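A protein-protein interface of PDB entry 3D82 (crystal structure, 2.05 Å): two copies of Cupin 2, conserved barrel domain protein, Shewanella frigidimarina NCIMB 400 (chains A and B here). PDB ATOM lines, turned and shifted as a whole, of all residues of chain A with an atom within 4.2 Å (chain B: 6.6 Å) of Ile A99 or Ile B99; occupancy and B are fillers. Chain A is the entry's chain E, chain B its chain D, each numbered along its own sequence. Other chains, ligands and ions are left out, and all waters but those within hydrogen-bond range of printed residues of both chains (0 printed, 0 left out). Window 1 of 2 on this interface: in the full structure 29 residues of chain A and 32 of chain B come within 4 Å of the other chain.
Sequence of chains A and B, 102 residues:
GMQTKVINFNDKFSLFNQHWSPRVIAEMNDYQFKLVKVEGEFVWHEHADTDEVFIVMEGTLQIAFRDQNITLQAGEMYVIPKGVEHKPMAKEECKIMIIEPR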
ATOM      1  N   MET A  28     -32.623  -5.976  10.403  1.00  0.00           N
ATOM      2  CA  MET A  28     -32.649  -7.400  10.670  1.00  0.00           C
ATOM      3  C   MET A  28     -32.116  -7.558  12.100  1.00  0.00           C
ATOM      4  O   MET A  28     -30.914  -7.371  12.335  1.00  0.00           O
ATOM      5  CB  MET A  28     -31.745  -8.131   9.692  1.00  0.00           C
ATOM      6  CG  MET A  28     -31.508  -9.608   9.993  1.00  0.00           C
ATOM      7  SD  MET A  28     -30.113 -10.351   8.860  1.00  0.00           S
ATOM      8  CE  MET A  28     -28.567  -9.194   9.433  1.00  0.00           C
ATOM      9  N   GLN A  32     -28.524  -3.165  10.581  1.00  0.00           N
ATOM     10  CA  GLN A  32     -29.082  -2.272   9.569  1.00  0.00           C
ATOM     11  C   GLN A  32     -28.458  -2.499   8.206  1.00  0.00           C
ATOM     12  O   GLN A  32     -27.264  -2.777   8.113  1.00  0.00           O
ATOM     13  CB  GLN A  32     -28.835  -0.839   9.949  1.00  0.00           C
ATOM     14  CG  GLN A  32     -29.662  -0.413  11.095  1.00  0.00           C
ATOM     15  CD  GLN A  32     -29.343   0.997  11.568  1.00  0.00           C
ATOM     16  OE1 GLN A  32     -28.192   1.441  11.567  1.00  0.00           O
ATOM     17  NE2 GLN A  32     -30.371   1.688  12.009  1.00  0.00           N
ATOM     18  N   PHE A  33     -29.289  -2.327   7.176  1.00  0.00           N
ATOM     19  CA  PHE A  33     -28.917  -2.390   5.763  1.00  0.00           C
ATOM     20  C   PHE A  33     -28.968  -0.943   5.321  1.00  0.00           C
ATOM     21  O   PHE A  33     -30.009  -0.273   5.481  1.00  0.00           O
ATOM     22  CB  PHE A  33     -29.919  -3.230   4.973  1.00  0.00           C
ATOM     23  CG  PHE A  33     -29.800  -4.697   5.228  1.00  0.00           C
ATOM     24  CD1 PHE A  33     -30.221  -5.242   6.438  1.00  0.00           C
ATOM     25  CD2 PHE A  33     -29.286  -5.553   4.255  1.00  0.00           C
ATOM     26  CE1 PHE A  33     -30.095  -6.587   6.685  1.00  0.00           C
ATOM     27  CE2 PHE A  33     -29.160  -6.915   4.496  1.00  0.00           C
ATOM     28  CZ  PHE A  33     -29.567  -7.427   5.723  1.00  0.00           C
ATOM     29  N   GLU A  52     -17.662  -5.538   9.132  1.00  0.00           N
ATOM     30  CA  GLU A  52     -18.479  -4.691   8.282  1.00  0.00           C
ATOM     31  C   GLU A  52     -18.501  -5.276   6.872  1.00  0.00           C
ATOM     32  O   GLU A  52     -17.470  -5.686   6.354  1.00  0.00           O
ATOM     33  CB  GLU A  52     -17.898  -3.284   8.227  1.00  0.00           C
ATOM     34  CG  GLU A  52     -18.760  -2.329   7.425  1.00  0.00           C
ATOM     35  CD  GLU A  52     -18.287  -0.920   7.532  1.00  0.00           C
ATOM     36  OE1 GLU A  52     -17.085  -0.674   7.273  1.00  0.00           O
ATOM     37  OE2 GLU A  52     -19.123  -0.060   7.835  1.00  0.00           O
ATOM     38  N   VAL A  53     -19.677  -5.287   6.256  1.00  0.00           N
ATOM     39  CA  VAL A  53     -19.872  -5.838   4.925  1.00  0.00           C
ATOM     40  C   VAL A  53     -20.102  -4.729   3.905  1.00  0.00           C
ATOM     41  O   VAL A  53     -20.901  -3.820   4.148  1.00  0.00           O
ATOM     42  CB  VAL A  53     -21.058  -6.852   4.916  1.00  0.00           C
ATOM     43  CG1 VAL A  53     -21.546  -7.184   3.474  1.00  0.00           C
ATOM     44  CG2 VAL A  53     -20.630  -8.146   5.633  1.00  0.00           C
ATOM     45  N   ILE A  55     -21.228  -4.477  -0.134  1.00  0.00           N
ATOM     46  CA  ILE A  55     -21.781  -5.110  -1.340  1.00  0.00           C
ATOM     47  C   ILE A  55     -21.840  -3.993  -2.393  1.00  0.00           C
ATOM     48  O   ILE A  55     -22.442  -2.944  -2.133  1.00  0.00           O
ATOM     49  CB  ILE A  55     -23.205  -5.701  -1.136  1.00  0.00           C
ATOM     50  CG1 ILE A  55     -23.216  -6.743  -0.014  1.00  0.00           C
ATOM     51  CG2 ILE A  55     -23.754  -6.350  -2.458  1.00  0.00           C
ATOM     52  CD1 ILE A  55     -24.592  -7.323   0.259  1.00  0.00           C
ATOM     53  N   ILE A  98     -24.121  -1.232   2.719  1.00  0.00           N
ATOM     54  CA  ILE A  98     -23.385  -1.573   3.912  1.00  0.00           C
ATOM     55  C   ILE A  98     -24.327  -2.277   4.884  1.00  0.00           C
ATOM     56  O   ILE A  98     -25.492  -1.907   4.996  1.00  0.00           O
ATOM     57  CB  ILE A  98     -22.737  -0.320   4.547  1.00  0.00           C
ATOM     58  CG1 ILE A  98     -21.563   0.133   3.669  1.00  0.00           C
ATOM     59  CG2 ILE A  98     -22.208  -0.620   5.926  1.00  0.00           C
ATOM     60  CD1 ILE A  98     -20.960   1.474   4.115  1.00  0.00           C
ATOM     61  N   ILE A  99     -23.803  -3.312   5.552  1.00  0.00           N
ATOM     62  CA  ILE A  99     -24.543  -4.071   6.555  1.00  0.00           C
ATOM     63  C   ILE A  99     -23.675  -4.121   7.803  1.00  0.00           C
ATOM     64  O   ILE A  99     -22.519  -4.544   7.732  1.00  0.00           O
ATOM     65  CB  ILE A  99     -24.881  -5.523   6.123  1.00  0.00           C
ATOM     66  CG1 ILE A  99     -25.531  -5.549   4.740  1.00  0.00           C
ATOM     67  CG2 ILE A  99     -25.813  -6.180   7.180  1.00  0.00           C
ATOM     68  CD1 ILE A  99     -25.658  -6.938   4.129  1.00  0.00           C
ATOM     69  N   GLU A 100     -24.234  -3.675   8.918  1.00  0.00           N
ATOM     70  CA  GLU A 100     -23.538  -3.636  10.179  1.00  0.00           C
ATOM     71  C   GLU A 100     -24.521  -3.491  11.355  1.00  0.00           C
ATOM     72  O   GLU A 100     -25.694  -3.114  11.149  1.00  0.00           O
ATOM     73  CB  GLU A 100     -22.556  -2.443  10.171  1.00  0.00           C
ATOM     74  CG  GLU A 100     -23.226  -1.070   9.983  1.00  0.00           C
ATOM     75  CD  GLU A 100     -22.234   0.091   9.696  1.00  0.00           C
ATOM     76  OE1 GLU A 100     -21.012  -0.121   9.781  1.00  0.00           O
ATOM     77  OE2 GLU A 100     -22.704   1.223   9.400  1.00  0.00           O
ATOM     78  N   MET B  28     -20.221 -12.612   8.871  1.00  0.00           N
ATOM     79  CA  MET B  28     -20.137 -11.278   9.480  1.00  0.00           C
ATOM     80  C   MET B  28     -20.508 -11.472  10.945  1.00  0.00           C
ATOM     81  O   MET B  28     -21.672 -11.691  11.252  1.00  0.00           O
ATOM     82  CB  MET B  28     -21.127 -10.321   8.810  1.00  0.00           C
ATOM     83  CG  MET B  28     -21.236  -8.941   9.471  1.00  0.00           C
ATOM     84  SD  MET B  28     -22.754  -7.975   8.729  1.00  0.00           S
ATOM     85  CE  MET B  28     -24.255  -9.101   9.185  1.00  0.00           C
ATOM     86  N   TYR B  31     -23.211 -13.993  11.998  1.00  0.00           N
ATOM     87  CA  TYR B  31     -24.177 -14.110  10.899  1.00  0.00           C
ATOM     88  C   TYR B  31     -23.526 -14.771   9.685  1.00  0.00           C
ATOM     89  O   TYR B  31     -22.301 -14.759   9.529  1.00  0.00           O
ATOM     90  CB  TYR B  31     -24.751 -12.734  10.522  1.00  0.00           C
ATOM     91  CG  TYR B  31     -25.789 -12.235  11.480  1.00  0.00           C
ATOM     92  CD1 TYR B  31     -25.446 -11.852  12.788  1.00  0.00           C
ATOM     93  CD2 TYR B  31     -27.140 -12.135  11.088  1.00  0.00           C
ATOM     94  CE1 TYR B  31     -26.436 -11.404  13.691  1.00  0.00           C
ATOM     95  CE2 TYR B  31     -28.122 -11.667  11.977  1.00  0.00           C
ATOM     96  CZ  TYR B  31     -27.764 -11.300  13.264  1.00  0.00           C
ATOM     97  OH  TYR B  31     -28.732 -10.877  14.121  1.00  0.00           O
ATOM     98  N   GLN B  32     -24.361 -15.372   8.847  1.00  0.00           N
ATOM     99  CA  GLN B  32     -23.928 -16.024   7.601  1.00  0.00           C
ATOM    100  C   GLN B  32     -24.716 -15.485   6.407  1.00  0.00           C
ATOM    101  O   GLN B  32     -25.905 -15.173   6.539  1.00  0.00           O
ATOM    102  CB  GLN B  32     -24.119 -17.520   7.707  1.00  0.00           C
ATOM    103  CG  GLN B  32     -23.164 -18.186   8.723  1.00  0.00           C
ATOM    104  CD  GLN B  32     -23.391 -19.659   8.859  1.00  0.00           C
ATOM    105  OE1 GLN B  32     -24.529 -20.129   8.806  1.00  0.00           O
ATOM    106  NE2 GLN B  32     -22.308 -20.411   9.050  1.00  0.00           N
ATOM    107  N   PHE B  33     -24.022 -15.342   5.277  1.00  0.00           N
ATOM    108  CA  PHE B  33     -24.610 -14.952   3.988  1.00  0.00           C
ATOM    109  C   PHE B  33     -24.623 -16.275   3.249  1.00  0.00           C
ATOM    110  O   PHE B  33     -23.584 -16.917   3.146  1.00  0.00           O
ATOM    111  CB  PHE B  33     -23.743 -13.933   3.249  1.00  0.00           C
ATOM    112  CG  PHE B  33     -23.747 -12.573   3.890  1.00  0.00           C
ATOM    113  CD1 PHE B  33     -23.101 -12.358   5.107  1.00  0.00           C
ATOM    114  CD2 PHE B  33     -24.393 -11.504   3.272  1.00  0.00           C
ATOM    115  CE1 PHE B  33     -23.131 -11.111   5.725  1.00  0.00           C
ATOM    116  CE2 PHE B  33     -24.405 -10.225   3.876  1.00  0.00           C
ATOM    117  CZ  PHE B  33     -23.784 -10.049   5.118  1.00  0.00           C
ATOM    118  N   LYS B  34     -25.789 -16.676   2.757  1.00  0.00           N
ATOM    119  CA  LYS B  34     -25.961 -17.982   2.119  1.00  0.00           C
ATOM    120  C   LYS B  34     -26.639 -17.827   0.780  1.00  0.00           C
ATOM    121  O   LYS B  34     -27.653 -17.145   0.689  1.00  0.00           O
ATOM    122  CB  LYS B  34     -26.820 -18.878   3.028  1.00  0.00           C
ATOM    123  CG  LYS B  34     -26.097 -19.314   4.303  1.00  0.00           C
ATOM    124  CD  LYS B  34     -26.958 -19.332   5.552  1.00  0.00           C
ATOM    125  CE  LYS B  34     -27.862 -20.497   5.721  1.00  0.00           C
ATOM    126  NZ  LYS B  34     -28.658 -20.315   7.016  1.00  0.00           N
ATOM    127  N   THR B  50     -35.284 -15.242  15.325  1.00  0.00           N
ATOM    128  CA  THR B  50     -34.562 -14.309  14.452  1.00  0.00           C
ATOM    129  C   THR B  50     -35.347 -13.854  13.231  1.00  0.00           C
ATOM    130  O   THR B  50     -36.121 -14.635  12.639  1.00  0.00           O
ATOM    131  CB  THR B  50     -33.187 -14.924  13.957  1.00  0.00           C
ATOM    132  OG1 THR B  50     -32.473 -13.944  13.189  1.00  0.00           O
ATOM    133  CG2 THR B  50     -33.389 -16.186  13.095  1.00  0.00           C
ATOM    134  N   ASP B  51     -35.117 -12.596  12.844  1.00  0.00           N
ATOM    135  CA  ASP B  51     -35.579 -12.105  11.550  1.00  0.00           C
ATOM    136  C   ASP B  51     -34.721 -12.857  10.493  1.00  0.00           C
ATOM    137  O   ASP B  51     -33.641 -13.349  10.801  1.00  0.00           O
ATOM    138  CB  ASP B  51     -35.343 -10.622  11.356  1.00  0.00           C
ATOM    139  CG  ASP B  51     -36.078  -9.760  12.359  1.00  0.00           C
ATOM    140  OD1 ASP B  51     -37.104 -10.184  12.926  1.00  0.00           O
ATOM    141  OD2 ASP B  51     -35.591  -8.638  12.568  1.00  0.00           O
ATOM    142  N   GLU B  52     -35.216 -12.920   9.270  1.00  0.00           N
ATOM    143  CA  GLU B  52     -34.530 -13.586   8.164  1.00  0.00           C
ATOM    144  C   GLU B  52     -34.667 -12.708   6.922  1.00  0.00           C
ATOM    145  O   GLU B  52     -35.777 -12.295   6.578  1.00  0.00           O
ATOM    146  CB  GLU B  52     -35.154 -14.962   7.912  1.00  0.00           C
ATOM    147  CG  GLU B  52     -34.467 -15.783   6.829  1.00  0.00           C
ATOM    148  CD  GLU B  52     -35.143 -17.120   6.628  1.00  0.00           C
ATOM    149  OE1 GLU B  52     -36.327 -17.117   6.266  1.00  0.00           O
ATOM    150  OE2 GLU B  52     -34.510 -18.185   6.811  1.00  0.00           O
ATOM    151  N   VAL B  53     -33.546 -12.445   6.256  1.00  0.00           N
ATOM    152  CA  VAL B  53     -33.512 -11.622   5.058  1.00  0.00           C
ATOM    153  C   VAL B  53     -33.414 -12.473   3.798  1.00  0.00           C
ATOM    154  O   VAL B  53     -32.645 -13.413   3.756  1.00  0.00           O
ATOM    155  CB  VAL B  53     -32.349 -10.592   5.123  1.00  0.00           C
ATOM    156  CG1 VAL B  53     -32.147  -9.861   3.756  1.00  0.00           C
ATOM    157  CG2 VAL B  53     -32.627  -9.570   6.248  1.00  0.00           C
ATOM    158  N   PHE B  54     -34.233 -12.134   2.800  1.00  0.00           N
ATOM    159  CA  PHE B  54     -34.178 -12.704   1.461  1.00  0.00           C
ATOM    160  C   PHE B  54     -33.816 -11.579   0.494  1.00  0.00           C
ATOM    161  O   PHE B  54     -34.433 -10.511   0.528  1.00  0.00           O
ATOM    162  CB  PHE B  54     -35.532 -13.250   1.015  1.00  0.00           C
ATOM    163  CG  PHE B  54     -35.894 -14.544   1.638  1.00  0.00           C
ATOM    164  CD1 PHE B  54     -36.412 -14.574   2.925  1.00  0.00           C
ATOM    165  CD2 PHE B  54     -35.761 -15.743   0.927  1.00  0.00           C
ATOM    166  CE1 PHE B  54     -36.760 -15.774   3.509  1.00  0.00           C
ATOM    167  CE2 PHE B  54     -36.101 -16.952   1.514  1.00  0.00           C
ATOM    168  CZ  PHE B  54     -36.605 -16.974   2.802  1.00  0.00           C
ATOM    169  N   ILE B  55     -32.820 -11.827  -0.345  1.00  0.00           N
ATOM    170  CA  ILE B  55     -32.435 -10.912  -1.413  1.00  0.00           C
ATOM    171  C   ILE B  55     -32.490 -11.769  -2.673  1.00  0.00           C
ATOM    172  O   ILE B  55     -31.860 -12.832  -2.724  1.00  0.00           O
ATOM    173  CB  ILE B  55     -31.027 -10.337  -1.223  1.00  0.00           C
ATOM    174  CG1 ILE B  55     -30.903  -9.614   0.134  1.00  0.00           C
ATOM    175  CG2 ILE B  55     -30.668  -9.373  -2.369  1.00  0.00           C
ATOM    176  CD1 ILE B  55     -29.504  -9.049   0.437  1.00  0.00           C
ATOM    177  N   MET B  97     -30.204 -14.982  -1.970  1.00  0.00           N
ATOM    178  CA  MET B  97     -29.269 -14.863  -0.886  1.00  0.00           C
ATOM    179  C   MET B  97     -30.082 -14.688   0.395  1.00  0.00           C
ATOM    180  O   MET B  97     -31.021 -13.895   0.430  1.00  0.00           O
ATOM    181  CB  MET B  97     -28.276 -13.700  -1.064  1.00  0.00           C
ATOM    182  CG  MET B  97     -27.250 -13.678   0.067  1.00  0.00           C
ATOM    183  SD  MET B  97     -25.640 -12.735  -0.318  1.00  0.00           S
ATOM    184  CE  MET B  97     -26.378 -10.993  -0.233  1.00  0.00           C
ATOM    185  N   ILE B  98     -29.733 -15.472   1.408  1.00  0.00           N
ATOM    186  CA  ILE B  98     -30.351 -15.417   2.736  1.00  0.00           C
ATOM    187  C   ILE B  98     -29.288 -14.982   3.728  1.00  0.00           C
ATOM    188  O   ILE B  98     -28.142 -15.433   3.641  1.00  0.00           O
ATOM    189  CB  ILE B  98     -30.920 -16.771   3.180  1.00  0.00           C
ATOM    190  CG1 ILE B  98     -32.087 -17.195   2.299  1.00  0.00           C
ATOM    191  CG2 ILE B  98     -31.431 -16.725   4.624  1.00  0.00           C
ATOM    192  CD1 ILE B  98     -32.424 -18.717   2.505  1.00  0.00           C
ATOM    193  N   ILE B  99     -29.674 -14.089   4.645  1.00  0.00           N
ATOM    194  CA  ILE B  99     -28.789 -13.595   5.685  1.00  0.00           C
ATOM    195  C   ILE B  99     -29.509 -13.800   7.008  1.00  0.00           C
ATOM    196  O   ILE B  99     -30.670 -13.382   7.169  1.00  0.00           O
ATOM    197  CB  ILE B  99     -28.410 -12.104   5.508  1.00  0.00           C
ATOM    198  CG1 ILE B  99     -27.925 -11.803   4.074  1.00  0.00           C
ATOM    199  CG2 ILE B  99     -27.315 -11.713   6.539  1.00  0.00           C
ATOM    200  CD1 ILE B  99     -27.723 -10.312   3.790  1.00  0.00           C
ATOM    201  N   GLU B 100     -28.834 -14.463   7.933  1.00  0.00           N
ATOM    202  CA  GLU B 100     -29.384 -14.762   9.250  1.00  0.00           C
ATOM    203  C   GLU B 100     -28.273 -15.262  10.183  1.00  0.00           C
ATOM    204  O   GLU B 100     -27.207 -15.672   9.691  1.00  0.00           O
ATOM    205  CB  GLU B 100     -30.498 -15.828   9.122  1.00  0.00           C
ATOM    206  CG  GLU B 100     -30.029 -17.202   8.568  1.00  0.00           C
ATOM    207  CD  GLU B 100     -31.214 -18.121   8.226  1.00  0.00           C
ATOM    208  OE1 GLU B 100     -32.376 -17.783   8.582  1.00  0.00           O
ATOM    209  OE2 GLU B 100     -30.978 -19.177   7.608  1.00  0.00           O
ATOM    210  N   PRO B 101     -28.528 -15.284  11.514  1.00  0.00           N
ATOM    211  CA  PRO B 101     -27.517 -15.762  12.459  1.00  0.00           C
ATOM    212  C   PRO B 101     -27.109 -17.191  12.189  1.00  0.00           C
ATOM    213  O   PRO B 101     -27.894 -17.951  11.611  1.00  0.00           O
ATOM    214  CB  PRO B 101     -28.234 -15.698  13.818  1.00  0.00           C
ATOM    215  CG  PRO B 101     -29.285 -14.697  13.638  1.00  0.00           C
ATOM    216  CD  PRO B 101     -29.748 -14.869  12.227  1.00  0.00           C
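The side-chain sulfur (SD) of Met A28 sits close to the backbone carbonyl oxygen (O) of Ile B99, 3.5 Å away.
O of Ile A99 lies close to SD of Met B28, at 3.6 Å.
N of Val B53 lies within hydrogen-bond range of O of Ile B99 (3.2 Å).
The backbone carbonyl oxygen of Val A53 lies within hydrogen-bond range of the backbone NH of Ile A99 (3.3 Å).
Among the printed residues, merely in contact across the chains: Ile A99 with Phe B33, Met A28 with Tyr B31, Met A28 with Asp B51, Met A28 with Val B53, Val A53 with Phe B33, Phe A33 with Ile B99, Val A53 with Met B28, Phe A33 with Val B53 and Ile A99 with Ile B99.
Of the printed residues of chain B, Met A28 touches Tyr B31 (3.6 Å), Asp B51 (3.7 Å), Val B53 (3.7 Å) and Ile B99 (3.5 Å).
Of the printed residues of chain B, Phe A33 touches Val B53 and Ile B99.
Ile A99 touches just these residues of chain B: Met B28, Phe B33 and Ile B99.
Ile B98 touches none of the printed residues of chain A.
Ile B99 touches just these residues of chain A: Met A28 (3.5 Å), Phe A33 (3.8 Å) and Ile A99 (3.97 Å).
The nearest residue of chain B that does not touch Ile A99 is Ile B55 (5.7 Å).
The nearest printed residue of chain A that does not touch Ile B99 is Ile A55 (5.6 Å).
The nearest printed residue of chain B that does not touch Met A28 is Met B28 (4.3 Å).
Of the 9 printed residues of chain A, 4 touch a printed residue of chain B.
Printed residues of chain B that touch a printed residue of chain A: Met B28, Tyr B31, Phe B33, Asp B51, Val B53 and Ile B99.
Hydrophobic or aromatic side chains of chain B that line the printed part of chain A: Met B28, Tyr B31, Phe B33, Val B53 and Ile B99.
Met A28 touches Ile B99, and with the chains exchanged Ile A99 touches Met B28.
Phe A33 touches Val B53, and with the chains exchanged Val A53 touches Phe B33.
Phe A33 touches Ile B99, and with the chains exchanged Ile A99 touches Phe B33.
Ile B99 touches its own counterpart, Ile A99.
9 positions are printed for both chains.
Of the 11 pairs that touch across the chains among the printed residues, 9 have their exchanged pair printed and touching as well.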
